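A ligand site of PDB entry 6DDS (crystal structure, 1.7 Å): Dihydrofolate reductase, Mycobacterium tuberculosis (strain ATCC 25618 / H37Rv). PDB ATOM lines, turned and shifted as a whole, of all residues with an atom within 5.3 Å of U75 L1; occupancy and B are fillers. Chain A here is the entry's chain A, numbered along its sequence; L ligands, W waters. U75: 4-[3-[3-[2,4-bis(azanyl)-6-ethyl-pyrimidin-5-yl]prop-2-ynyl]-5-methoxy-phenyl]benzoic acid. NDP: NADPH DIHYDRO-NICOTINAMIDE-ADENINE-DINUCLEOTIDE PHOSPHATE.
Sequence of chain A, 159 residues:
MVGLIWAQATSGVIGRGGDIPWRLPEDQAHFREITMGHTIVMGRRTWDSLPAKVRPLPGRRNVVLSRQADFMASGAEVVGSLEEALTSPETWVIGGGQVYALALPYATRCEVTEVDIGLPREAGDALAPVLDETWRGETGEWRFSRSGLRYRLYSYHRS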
ATOM      1  N   ILE A   5       9.695 -22.246  24.340  1.00  0.00           N
ATOM      2  CA  ILE A   5      10.076 -22.921  23.100  1.00  0.00           C
ATOM      3  C   ILE A   5      10.547 -21.868  22.125  1.00  0.00           C
ATOM      4  O   ILE A   5       9.885 -20.834  21.933  1.00  0.00           O
ATOM      5  CB  ILE A   5       8.912 -23.801  22.514  1.00  0.00           C
ATOM      6  CG1 ILE A   5       9.309 -24.446  21.183  1.00  0.00           C
ATOM      7  CG2 ILE A   5       7.612 -23.013  22.376  1.00  0.00           C
ATOM      8  CD1 ILE A   5       8.276 -25.485  20.719  1.00  0.00           C
ATOM      9  N   TRP A   6      11.734 -22.094  21.546  1.00  0.00           N
ATOM     10  CA  TRP A   6      12.285 -21.186  20.558  1.00  0.00           C
ATOM     11  C   TRP A   6      13.244 -21.888  19.595  1.00  0.00           C
ATOM     12  O   TRP A   6      13.691 -23.005  19.873  1.00  0.00           O
ATOM     13  CB  TRP A   6      13.023 -20.023  21.242  1.00  0.00           C
ATOM     14  CG  TRP A   6      14.364 -20.348  21.868  1.00  0.00           C
ATOM     15  CD1 TRP A   6      15.586 -20.394  21.224  1.00  0.00           C
ATOM     16  CD2 TRP A   6      14.638 -20.577  23.250  1.00  0.00           C
ATOM     17  NE1 TRP A   6      16.579 -20.678  22.134  1.00  0.00           N
ATOM     18  CE2 TRP A   6      16.031 -20.774  23.381  1.00  0.00           C
ATOM     19  CE3 TRP A   6      13.847 -20.627  24.410  1.00  0.00           C
ATOM     20  CZ2 TRP A   6      16.645 -21.053  24.609  1.00  0.00           C
ATOM     21  CZ3 TRP A   6      14.457 -20.898  25.635  1.00  0.00           C
ATOM     22  CH2 TRP A   6      15.855 -21.097  25.725  1.00  0.00           C
ATOM     23  N   ALA A   7      13.516 -21.221  18.475  1.00  0.00           N
ATOM     24  CA  ALA A   7      14.556 -21.634  17.536  1.00  0.00           C
ATOM     25  C   ALA A   7      15.600 -20.533  17.480  1.00  0.00           C
ATOM     26  O   ALA A   7      15.274 -19.353  17.355  1.00  0.00           O
ATOM     27  CB  ALA A   7      13.984 -21.888  16.150  1.00  0.00           C
ATOM     28  N   ILE A  20      12.062 -13.778  11.860  1.00  0.00           N
ATOM     29  CA  ILE A  20      12.968 -14.878  12.146  1.00  0.00           C
ATOM     30  C   ILE A  20      13.911 -14.996  10.946  1.00  0.00           C
ATOM     31  O   ILE A  20      13.464 -15.259   9.821  1.00  0.00           O
ATOM     32  CB  ILE A  20      12.198 -16.193  12.421  1.00  0.00           C
ATOM     33  CG1 ILE A  20      11.286 -16.029  13.638  1.00  0.00           C
ATOM     34  CG2 ILE A  20      13.160 -17.360  12.622  1.00  0.00           C
ATOM     35  CD1 ILE A  20      10.395 -17.247  13.917  1.00  0.00           C
ATOM     36  N   ASP A  27      11.141 -27.100  11.547  1.00  0.00           N
ATOM     37  CA  ASP A  27      11.012 -26.531  12.894  1.00  0.00           C
ATOM     38  C   ASP A  27       9.553 -26.189  13.187  1.00  0.00           C
ATOM     39  O   ASP A  27       9.071 -26.421  14.287  1.00  0.00           O
ATOM     40  CB  ASP A  27      11.892 -25.293  13.045  1.00  0.00           C
ATOM     41  CG  ASP A  27      11.661 -24.577  14.377  1.00  0.00           C
ATOM     42  OD1 ASP A  27      11.945 -25.162  15.436  1.00  0.00           O
ATOM     43  OD2 ASP A  27      11.228 -23.404  14.334  1.00  0.00           O
ATOM     44  N   GLN A  28       8.856 -25.635  12.201  1.00  0.00           N
ATOM     45  CA  GLN A  28       7.430 -25.355  12.392  1.00  0.00           C
ATOM     46  C   GLN A  28       6.648 -26.594  12.835  1.00  0.00           C
ATOM     47  O   GLN A  28       5.779 -26.510  13.721  1.00  0.00           O
ATOM     48  CB  GLN A  28       6.806 -24.793  11.112  1.00  0.00           C
ATOM     49  CG  GLN A  28       5.331 -24.443  11.302  1.00  0.00           C
ATOM     50  CD  GLN A  28       4.770 -23.659  10.135  1.00  0.00           C
ATOM     51  OE1 GLN A  28       5.192 -22.527   9.865  1.00  0.00           O
ATOM     52  NE2 GLN A  28       3.816 -24.252   9.446  1.00  0.00           N
ATOM     53  N   HIS A  30       7.764 -29.261  14.368  1.00  0.00           N
ATOM     54  CA  HIS A  30       8.179 -29.558  15.732  1.00  0.00           C
ATOM     55  C   HIS A  30       7.471 -28.628  16.716  1.00  0.00           C
ATOM     56  O   HIS A  30       6.993 -29.046  17.764  1.00  0.00           O
ATOM     57  CB  HIS A  30       9.701 -29.421  15.853  1.00  0.00           C
ATOM     58  CG  HIS A  30      10.199 -29.500  17.272  1.00  0.00           C
ATOM     59  ND1 HIS A  30      10.888 -28.463  17.883  1.00  0.00           N
ATOM     60  CD2 HIS A  30      10.108 -30.485  18.187  1.00  0.00           C
ATOM     61  CE1 HIS A  30      11.199 -28.818  19.118  1.00  0.00           C
ATOM     62  NE2 HIS A  30      10.741 -30.041  19.329  1.00  0.00           N
ATOM     63  N   PHE A  31       7.437 -27.352  16.361  1.00  0.00           N
ATOM     64  CA  PHE A  31       6.780 -26.339  17.195  1.00  0.00           C
ATOM     65  C   PHE A  31       5.314 -26.681  17.373  1.00  0.00           C
ATOM     66  O   PHE A  31       4.767 -26.600  18.472  1.00  0.00           O
ATOM     67  CB  PHE A  31       6.959 -24.958  16.554  1.00  0.00           C
ATOM     68  CG  PHE A  31       6.120 -23.880  17.161  1.00  0.00           C
ATOM     69  CD1 PHE A  31       6.590 -23.123  18.246  1.00  0.00           C
ATOM     70  CD2 PHE A  31       4.847 -23.599  16.662  1.00  0.00           C
ATOM     71  CE1 PHE A  31       5.827 -22.130  18.790  1.00  0.00           C
ATOM     72  CE2 PHE A  31       4.079 -22.598  17.203  1.00  0.00           C
ATOM     73  CZ  PHE A  31       4.571 -21.858  18.277  1.00  0.00           C
ATOM     74  N   ARG A  32       4.674 -27.099  16.274  1.00  0.00           N
ATOM     75  CA  ARG A  32       3.239 -27.387  16.315  1.00  0.00           C
ATOM     76  C   ARG A  32       2.951 -28.590  17.199  1.00  0.00           C
ATOM     77  O   ARG A  32       1.961 -28.611  17.923  1.00  0.00           O
ATOM     78  CB  ARG A  32       2.697 -27.626  14.902  1.00  0.00           C
ATOM     79  CG  ARG A  32       1.188 -27.889  14.862  1.00  0.00           C
ATOM     80  CD  ARG A  32       0.708 -28.362  13.500  1.00  0.00           C
ATOM     81  NE  ARG A  32       0.748 -27.307  12.498  1.00  0.00           N
ATOM     82  CZ  ARG A  32       0.617 -27.527  11.186  1.00  0.00           C
ATOM     83  NH1 ARG A  32       0.464 -28.765  10.741  1.00  0.00           N
ATOM     84  NH2 ARG A  32       0.653 -26.518  10.336  1.00  0.00           N
ATOM     85  N   MET A  36       0.453 -27.773  20.260  1.00  0.00           N
ATOM     86  CA  MET A  36      -0.935 -28.050  19.902  1.00  0.00           C
ATOM     87  C   MET A  36      -1.791 -28.434  21.109  1.00  0.00           C
ATOM     88  O   MET A  36      -1.405 -29.287  21.918  1.00  0.00           O
ATOM     89  CB  MET A  36      -0.998 -29.166  18.845  1.00  0.00           C
ATOM     90  CG  MET A  36      -2.403 -29.413  18.292  1.00  0.00           C
ATOM     91  SD  MET A  36      -3.134 -27.931  17.544  1.00  0.00           S
ATOM     92  CE  MET A  36      -1.747 -27.300  16.641  1.00  0.00           C
ATOM     93  N   THR A  46       5.428 -10.404  18.898  1.00  0.00           N
ATOM     94  CA  THR A  46       5.398 -11.737  18.309  1.00  0.00           C
ATOM     95  C   THR A  46       4.009 -12.010  17.735  1.00  0.00           C
ATOM     96  O   THR A  46       3.884 -12.582  16.655  1.00  0.00           O
ATOM     97  CB  THR A  46       5.801 -12.794  19.352  1.00  0.00           C
ATOM     98  OG1 THR A  46       7.212 -12.686  19.593  1.00  0.00           O
ATOM     99  CG2 THR A  46       5.490 -14.216  18.855  1.00  0.00           C
ATOM    100  N   SER A  49       3.739 -10.453  14.394  1.00  0.00           N
ATOM    101  CA  SER A  49       4.544 -11.129  13.361  1.00  0.00           C
ATOM    102  C   SER A  49       3.874 -12.374  12.773  1.00  0.00           C
ATOM    103  O   SER A  49       4.293 -12.859  11.713  1.00  0.00           O
ATOM    104  CB  SER A  49       5.915 -11.499  13.933  1.00  0.00           C
ATOM    105  OG  SER A  49       5.890 -12.747  14.597  1.00  0.00           O
ATOM    106  N   LEU A  50       2.866 -12.902  13.445  1.00  0.00           N
ATOM    107  CA  LEU A  50       2.149 -14.050  12.913  1.00  0.00           C
ATOM    108  C   LEU A  50       1.463 -13.703  11.593  1.00  0.00           C
ATOM    109  O   LEU A  50       0.738 -12.701  11.512  1.00  0.00           O
ATOM    110  CB  LEU A  50       1.112 -14.547  13.923  1.00  0.00           C
ATOM    111  CG  LEU A  50       1.617 -15.088  15.252  1.00  0.00           C
ATOM    112  CD1 LEU A  50       0.420 -15.471  16.123  1.00  0.00           C
ATOM    113  CD2 LEU A  50       2.523 -16.284  15.050  1.00  0.00           C
ATOM    114  N   PRO A  51       1.676 -14.530  10.557  1.00  0.00           N
ATOM    115  CA  PRO A  51       0.915 -14.355   9.310  1.00  0.00           C
ATOM    116  C   PRO A  51      -0.594 -14.345   9.610  1.00  0.00           C
ATOM    117  O   PRO A  51      -1.047 -15.111  10.453  1.00  0.00           O
ATOM    118  CB  PRO A  51       1.311 -15.586   8.491  1.00  0.00           C
ATOM    119  CG  PRO A  51       2.649 -15.995   9.034  1.00  0.00           C
ATOM    120  CD  PRO A  51       2.577 -15.686  10.514  1.00  0.00           C
ATOM    121  N   VAL A  54      -2.797 -17.413  10.038  1.00  0.00           N
ATOM    122  CA  VAL A  54      -2.647 -18.203  11.249  1.00  0.00           C
ATOM    123  C   VAL A  54      -2.525 -17.317  12.485  1.00  0.00           C
ATOM    124  O   VAL A  54      -1.749 -17.605  13.414  1.00  0.00           O
ATOM    125  CB  VAL A  54      -1.425 -19.143  11.174  1.00  0.00           C
ATOM    126  CG1 VAL A  54      -1.645 -20.202  10.124  1.00  0.00           C
ATOM    127  CG2 VAL A  54      -0.177 -18.331  10.869  1.00  0.00           C
ATOM    128  N   LEU A  57      -3.022 -18.576  16.163  1.00  0.00           N
ATOM    129  CA  LEU A  57      -2.597 -19.935  15.829  1.00  0.00           C
ATOM    130  C   LEU A  57      -3.685 -20.915  16.225  1.00  0.00           C
ATOM    131  O   LEU A  57      -4.068 -21.002  17.384  1.00  0.00           O
ATOM    132  CB  LEU A  57      -1.280 -20.273  16.539  1.00  0.00           C
ATOM    133  CG  LEU A  57      -0.037 -19.606  15.951  1.00  0.00           C
ATOM    134  CD1 LEU A  57       1.141 -19.716  16.914  1.00  0.00           C
ATOM    135  CD2 LEU A  57       0.320 -20.261  14.614  1.00  0.00           C
ATOM    136  N   ARG A  60      -4.783 -23.748  19.588  1.00  0.00           N
ATOM    137  CA  ARG A  60      -4.044 -23.252  20.754  1.00  0.00           C
ATOM    138  C   ARG A  60      -4.714 -22.014  21.316  1.00  0.00           C
ATOM    139  O   ARG A  60      -5.209 -21.181  20.560  1.00  0.00           O
ATOM    140  CB  ARG A  60      -2.588 -22.938  20.378  1.00  0.00           C
ATOM    141  CG  ARG A  60      -1.744 -24.190  20.176  1.00  0.00           C
ATOM    142  CD  ARG A  60      -0.683 -24.002  19.111  1.00  0.00           C
ATOM    143  NE  ARG A  60      -1.257 -23.965  17.770  1.00  0.00           N
ATOM    144  CZ  ARG A  60      -0.554 -24.057  16.661  1.00  0.00           C
ATOM    145  NH1 ARG A  60       0.770 -24.197  16.725  1.00  0.00           N
ATOM    146  NH2 ARG A  60      -1.162 -24.030  15.475  1.00  0.00           N
ATOM    147  N   VAL A  93       5.516 -20.689  26.373  1.00  0.00           N
ATOM    148  CA  VAL A  93       5.890 -19.337  25.973  1.00  0.00           C
ATOM    149  C   VAL A  93       6.615 -19.405  24.637  1.00  0.00           C
ATOM    150  O   VAL A  93       7.647 -20.071  24.530  1.00  0.00           O
ATOM    151  CB  VAL A  93       6.789 -18.674  27.037  1.00  0.00           C
ATOM    152  CG1 VAL A  93       7.152 -17.253  26.614  1.00  0.00           C
ATOM    153  CG2 VAL A  93       6.070 -18.660  28.379  1.00  0.00           C
ATOM    154  N   ILE A  94       6.065 -18.716  23.630  1.00  0.00           N
ATOM    155  CA  ILE A  94       6.557 -18.874  22.269  1.00  0.00           C
ATOM    156  C   ILE A  94       7.272 -17.621  21.740  1.00  0.00           C
ATOM    157  O   ILE A  94       7.509 -17.507  20.535  1.00  0.00           O
ATOM    158  CB  ILE A  94       5.405 -19.234  21.289  1.00  0.00           C
ATOM    159  CG1 ILE A  94       4.428 -18.060  21.092  1.00  0.00           C
ATOM    160  CG2 ILE A  94       4.647 -20.428  21.811  1.00  0.00           C
ATOM    161  CD1 ILE A  94       3.638 -18.152  19.754  1.00  0.00           C
ATOM    162  N   GLY A  95       7.610 -16.709  22.639  1.00  0.00           N
ATOM    163  CA  GLY A  95       8.383 -15.530  22.264  1.00  0.00           C
ATOM    164  C   GLY A  95       7.733 -14.196  22.579  1.00  0.00           C
ATOM    165  O   GLY A  95       6.605 -14.146  23.064  1.00  0.00           O
ATOM    166  N   TYR A 100      10.556 -14.096  26.774  1.00  0.00           N
ATOM    167  CA  TYR A 100      11.358 -15.202  27.313  1.00  0.00           C
ATOM    168  C   TYR A 100      12.071 -14.744  28.591  1.00  0.00           C
ATOM    169  O   TYR A 100      12.062 -15.452  29.587  1.00  0.00           O
ATOM    170  CB  TYR A 100      12.403 -15.719  26.319  1.00  0.00           C
ATOM    171  CG  TYR A 100      11.860 -16.417  25.091  1.00  0.00           C
ATOM    172  CD1 TYR A 100      10.920 -17.425  25.190  1.00  0.00           C
ATOM    173  CD2 TYR A 100      12.322 -16.074  23.825  1.00  0.00           C
ATOM    174  CE1 TYR A 100      10.429 -18.070  24.057  1.00  0.00           C
ATOM    175  CE2 TYR A 100      11.837 -16.690  22.696  1.00  0.00           C
ATOM    176  CZ  TYR A 100      10.904 -17.690  22.805  1.00  0.00           C
ATOM    177  OH  TYR A 100      10.434 -18.285  21.652  1.00  0.00           O
ATOM    178  N   GLU A 111      12.345 -26.110  25.128  1.00  0.00           N
ATOM    179  CA  GLU A 111      12.487 -26.900  23.923  1.00  0.00           C
ATOM    180  C   GLU A 111      13.126 -26.000  22.896  1.00  0.00           C
ATOM    181  O   GLU A 111      12.528 -25.015  22.456  1.00  0.00           O
ATOM    182  CB  GLU A 111      11.140 -27.437  23.436  1.00  0.00           C
ATOM    183  CG  GLU A 111      10.559 -28.508  24.355  1.00  0.00           C
ATOM    184  CD  GLU A 111      11.422 -29.768  24.450  1.00  0.00           C
ATOM    185  OE1 GLU A 111      12.241 -30.030  23.538  1.00  0.00           O
ATOM    186  OE2 GLU A 111      11.273 -30.512  25.442  1.00  0.00           O
ATOM    187  N   THR A 113      15.359 -25.356  19.312  1.00  0.00           N
ATOM    188  CA  THR A 113      15.887 -25.764  18.023  1.00  0.00           C
ATOM    189  C   THR A 113      17.122 -24.930  17.729  1.00  0.00           C
ATOM    190  O   THR A 113      17.023 -23.703  17.704  1.00  0.00           O
ATOM    191  CB  THR A 113      14.861 -25.543  16.887  1.00  0.00           C
ATOM    192  OG1 THR A 113      13.638 -26.231  17.173  1.00  0.00           O
ATOM    193  CG2 THR A 113      15.429 -26.015  15.540  1.00  0.00           C
HETATM  194  C4  U75 L   1       9.203 -21.101  16.027  1.00  0.00           C
HETATM  195  C5  U75 L   1       8.698 -20.350  17.084  1.00  0.00           C
HETATM  196  C6  U75 L   1       9.005 -20.769  18.369  1.00  0.00           C
HETATM  197  N1  U75 L   1       9.765 -21.855  18.548  1.00  0.00           N
HETATM  198  N3  U75 L   1       9.973 -22.172  16.258  1.00  0.00           N
HETATM  199  CAI U75 L   1       8.011 -21.789  14.080  1.00  0.00           C
HETATM  200  CAH U75 L   1       8.914 -20.728  14.696  1.00  0.00           C
HETATM  201  C2  U75 L   1      10.255 -22.541  17.522  1.00  0.00           C
HETATM  202  NAJ U75 L   1      10.998 -23.608  17.766  1.00  0.00           N
HETATM  203  NAG U75 L   1       8.545 -20.080  19.423  1.00  0.00           N
HETATM  204  CAK U75 L   1       7.895 -19.230  16.809  1.00  0.00           C
HETATM  205  CAL U75 L   1       7.225 -18.300  16.462  1.00  0.00           C
HETATM  206  CAM U75 L   1       6.400 -17.193  15.927  1.00  0.00           C
HETATM  207  CAN U75 L   1       5.913 -17.589  14.670  1.00  0.00           C
HETATM  208  CAO U75 L   1       5.116 -18.744  14.505  1.00  0.00           C
HETATM  209  CAS U75 L   1       6.234 -16.805  13.573  1.00  0.00           C
HETATM  210  CAR U75 L   1       5.775 -17.166  12.312  1.00  0.00           C
HETATM  211  OBB U75 L   1       6.112 -16.375  11.238  1.00  0.00           O
HETATM  212  CBC U75 L   1       6.432 -15.044  11.678  1.00  0.00           C
HETATM  213  CAQ U75 L   1       4.990 -18.302  12.145  1.00  0.00           C
HETATM  214  CAP U75 L   1       4.665 -19.118  13.229  1.00  0.00           C
HETATM  215  CAT U75 L   1       3.859 -20.256  13.057  1.00  0.00           C
HETATM  216  CAU U75 L   1       3.912 -21.334  13.951  1.00  0.00           C
HETATM  217  CAV U75 L   1       3.069 -22.448  13.795  1.00  0.00           C
HETATM  218  CAW U75 L   1       2.177 -22.511  12.732  1.00  0.00           C
HETATM  219  CAZ U75 L   1       1.333 -23.625  12.576  1.00  0.00           C
HETATM  220  OBD U75 L   1       0.730 -23.840  11.493  1.00  0.00           O
HETATM  221  OBA U75 L   1       1.146 -24.398  13.544  1.00  0.00           O
HETATM  222  CAX U75 L   1       2.125 -21.439  11.852  1.00  0.00           C
HETATM  223  CAY U75 L   1       2.947 -20.326  12.003  1.00  0.00           C
HETATM  224  PA  NDP L   2       8.103  -9.613  22.158  1.00  0.00           P
HETATM  225  O1A NDP L   2       8.708 -10.176  23.402  1.00  0.00           O
HETATM  226  O2A NDP L   2       7.589 -10.523  21.074  1.00  0.00           O
HETATM  227  O5B NDP L   2       6.808  -8.663  22.544  1.00  0.00           O
HETATM  228  C5B NDP L   2       7.260  -7.553  23.297  1.00  0.00           C
HETATM  229  C4B NDP L   2       5.993  -6.818  23.763  1.00  0.00           C
HETATM  230  O4B NDP L   2       5.373  -7.567  24.815  1.00  0.00           O
HETATM  231  C3B NDP L   2       6.238  -5.396  24.339  1.00  0.00           C
HETATM  232  O3B NDP L   2       6.338  -4.487  23.287  1.00  0.00           O
HETATM  233  C2B NDP L   2       4.871  -5.226  25.081  1.00  0.00           C
HETATM  234  O2B NDP L   2       3.832  -5.107  24.260  1.00  0.00           O
HETATM  235  C1B NDP L   2       4.738  -6.667  25.698  1.00  0.00           C
HETATM  236  N9A NDP L   2       5.379  -6.821  26.994  1.00  0.00           N
HETATM  237  C8A NDP L   2       6.743  -7.077  27.274  1.00  0.00           C
HETATM  238  N7A NDP L   2       7.001  -7.159  28.598  1.00  0.00           N
HETATM  239  C5A NDP L   2       5.730  -6.948  29.182  1.00  0.00           C
HETATM  240  C6A NDP L   2       5.299  -6.920  30.532  1.00  0.00           C
HETATM  241  N6A NDP L   2       6.184  -7.113  31.559  1.00  0.00           N
HETATM  242  N1A NDP L   2       3.984  -6.701  30.844  1.00  0.00           N
HETATM  243  C2A NDP L   2       3.144  -6.518  29.767  1.00  0.00           C
HETATM  244  N3A NDP L   2       3.398  -6.500  28.455  1.00  0.00           N
HETATM  245  C4A NDP L   2       4.731  -6.739  28.185  1.00  0.00           C
HETATM  246  O3  NDP L   2       9.120  -8.449  21.487  1.00  0.00           O
HETATM  247  PN  NDP L   2      10.616  -8.868  21.022  1.00  0.00           P
HETATM  248  O1N NDP L   2      11.010  -7.823  20.062  1.00  0.00           O
HETATM  249  O2N NDP L   2      11.551  -9.256  22.151  1.00  0.00           O
HETATM  250  O5D NDP L   2      10.656 -10.298  20.061  1.00  0.00           O
HETATM  251  C5D NDP L   2      10.233 -10.045  18.772  1.00  0.00           C
HETATM  252  C4D NDP L   2      11.224 -10.771  17.856  1.00  0.00           C
HETATM  253  O4D NDP L   2      11.322 -12.158  18.271  1.00  0.00           O
HETATM  254  C3D NDP L   2      10.742 -10.776  16.390  1.00  0.00           C
HETATM  255  O3D NDP L   2      11.868 -10.528  15.593  1.00  0.00           O
HETATM  256  C2D NDP L   2      10.267 -12.208  16.207  1.00  0.00           C
HETATM  257  O2D NDP L   2      10.449 -12.672  14.908  1.00  0.00           O
HETATM  258  C1D NDP L   2      11.291 -12.931  17.112  1.00  0.00           C
HETATM  259  N1N NDP L   2      10.778 -14.273  17.473  1.00  0.00           N
HETATM  260  C2N NDP L   2      11.575 -15.398  17.287  1.00  0.00           C
HETATM  261  C3N NDP L   2      11.169 -16.605  17.787  1.00  0.00           C
HETATM  262  C7N NDP L   2      12.002 -17.770  17.578  1.00  0.00           C
HETATM  263  O7N NDP L   2      11.766 -18.859  18.131  1.00  0.00           O
HETATM  264  N7N NDP L   2      13.109 -17.673  16.755  1.00  0.00           N
HETATM  265  C4N NDP L   2       9.901 -16.754  18.561  1.00  0.00           C
HETATM  266  C5N NDP L   2       9.079 -15.544  18.555  1.00  0.00           C
HETATM  267  C6N NDP L   2       9.502 -14.386  18.031  1.00  0.00           C
HETATM  268  P2B NDP L   2       3.194  -3.422  23.973  1.00  0.00           P
HETATM  269  O1X NDP L   2       4.413  -2.864  23.293  1.00  0.00           O
HETATM  270  O2X NDP L   2       1.975  -3.695  23.079  1.00  0.00           O
HETATM  271  O3X NDP L   2       2.948  -3.011  25.389  1.00  0.00           O
HETATM  272  O   HOH W   1      12.146 -25.789  19.543  1.00  0.00           O
HETATM  273  O   HOH W   2       0.599 -23.248   8.960  1.00  0.00           O
HETATM  274  O   HOH W   3      -1.826 -24.539  12.476  1.00  0.00           O
HETATM  275  O   HOH W   4       8.128 -14.197  14.634  1.00  0.00           O
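The side-chain carboxylate (OD2) of Asp 27 sits at hydrogen-bond distance from a nitrogen (N3) of U75 L1 (2.6 Å).
NH2 of Arg 32 lies within salt-bridge range of OBD of U75 L1 (2.9 Å).
The backbone carbonyl oxygen of Ile 5 is in hydrogen-bond range of a nitrogen (NAG) of U75 L1.
The backbone carbonyl oxygen of Ile 94 lies within hydrogen-bond range of a nitrogen (NAG) of U75 L1 (3.0 Å).
OBA of U75 L1 lies within salt-bridge range of NH2 of Arg 60 (3.0 Å).
The backbone carbonyl oxygen (O) of Trp 6 lies close to a nitrogen (NAJ) of U75 L1, at 3.5 Å.
NAG of U75 L1 lies within hydrogen-bond range of OH of Tyr 100, at 3.4 Å.
An oxygen (O7N) of NDP L2 is in hydrogen-bond range of the backbone NH (N) of Ala 7 (3.0 Å).
The backbone carbonyl oxygen (O) of Ala 7 sits at hydrogen-bond distance from a nitrogen (N7N) of NDP L2 (2.8 Å).
An oxygen (O2A) of NDP L2 is in hydrogen-bond range of the backbone NH (N) of Thr 46, 3.1 Å away.
An oxygen (O2A) of NDP L2 lies within hydrogen-bond range of the side-chain hydroxyl (OG1) of Thr 46 (2.6 Å).
The side-chain carboxylate (OD1) of Asp 27 is in hydrogen-bond range of the side-chain hydroxyl (OG1) of Thr 113 (2.7 Å).
O of Ile 5 is in hydrogen-bond range of OH of Tyr 100 (2.6 Å).
O of Val 93 sits at hydrogen-bond distance from N of Ile 5 (3.0 Å).
O of Ile 94 sits at hydrogen-bond distance from OH of Tyr 100 (3.2 Å).
O of Thr 46 lies within hydrogen-bond range of OG of Ser 49.
The backbone carbonyl oxygen (O) of Trp 6 is in hydrogen-bond range of the backbone NH (N) of Thr 113 (2.9 Å).
The backbone NH (N) of Trp 6 lies within hydrogen-bond range of the backbone carbonyl oxygen (O) of Glu 111 (3.2 Å).
The side-chain hydroxyl (OH) of Tyr 100 sits at hydrogen-bond distance from the backbone NH (N) of Gly 95 (3.4 Å).
Ala 7 touches U75 L1.
Ile 20 touches U75 L1 (CD1 to CAH, 3.9 Å).
Gln 28 touches U75 L1.
Phe 31 touches U75 L1 (CD1 to C6, 3.4 Å).
O of Ser 49 touches CBC of U75 L1 (3.1 Å).
Leu 50 touches U75 L1 (CD2 to CAO, 3.6 Å).
CD of Pro 51 touches OBB of U75 L1, at 3.7 Å.
CG2 of Val 54 touches CAY of U75 L1, at 3.9 Å.
Leu 57 touches U75 L1.
Thr 113 touches U75 L1 (OG1 to NAJ, 3.8 Å).
Hydrophobic or aromatic side chains that line U75 L1: Ile 5, Ala 7, Ile 20, Phe 31, Leu 50, Pro 51, Val 54, Leu 57 and Ile 94.
17 residues have an atom within 4 Å of U75 L1: Ile 5, Trp 6, Ala 7, Ile 20, Asp 27, Gln 28, Phe 31, Arg 32, Ser 49, Leu 50, Pro 51, Val 54, Leu 57, Arg 60, Ile 94, Tyr 100 and Thr 113.
Along chain A the residues within 4 Å of U75 L1 span positions 5 to 113.
The nearest printed residue that does not touch U75 L1 is Thr 46 (4.3 Å).
Water W2 bridges an oxygen (OBD) of U75 L1 and the side-chain amide nitrogen of Gln 28.
Water W3 bridges OBD of U75 L1 (2.8 Å) and NH2 of Arg 60 (3.1 Å).
Water W1 lies within hydrogen-bond range of OG1 of Thr 113 (2.8 Å), NAJ of U75 L1 (3.0 Å), O of Glu 111 (3.0 Å), O of Trp 6 (3.2 Å) and ND1 of His 30 (3.4 Å).
Water W4 bridges OG of Ser 49 (2.7 Å) and O2D of NDP L2 (2.8 Å).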
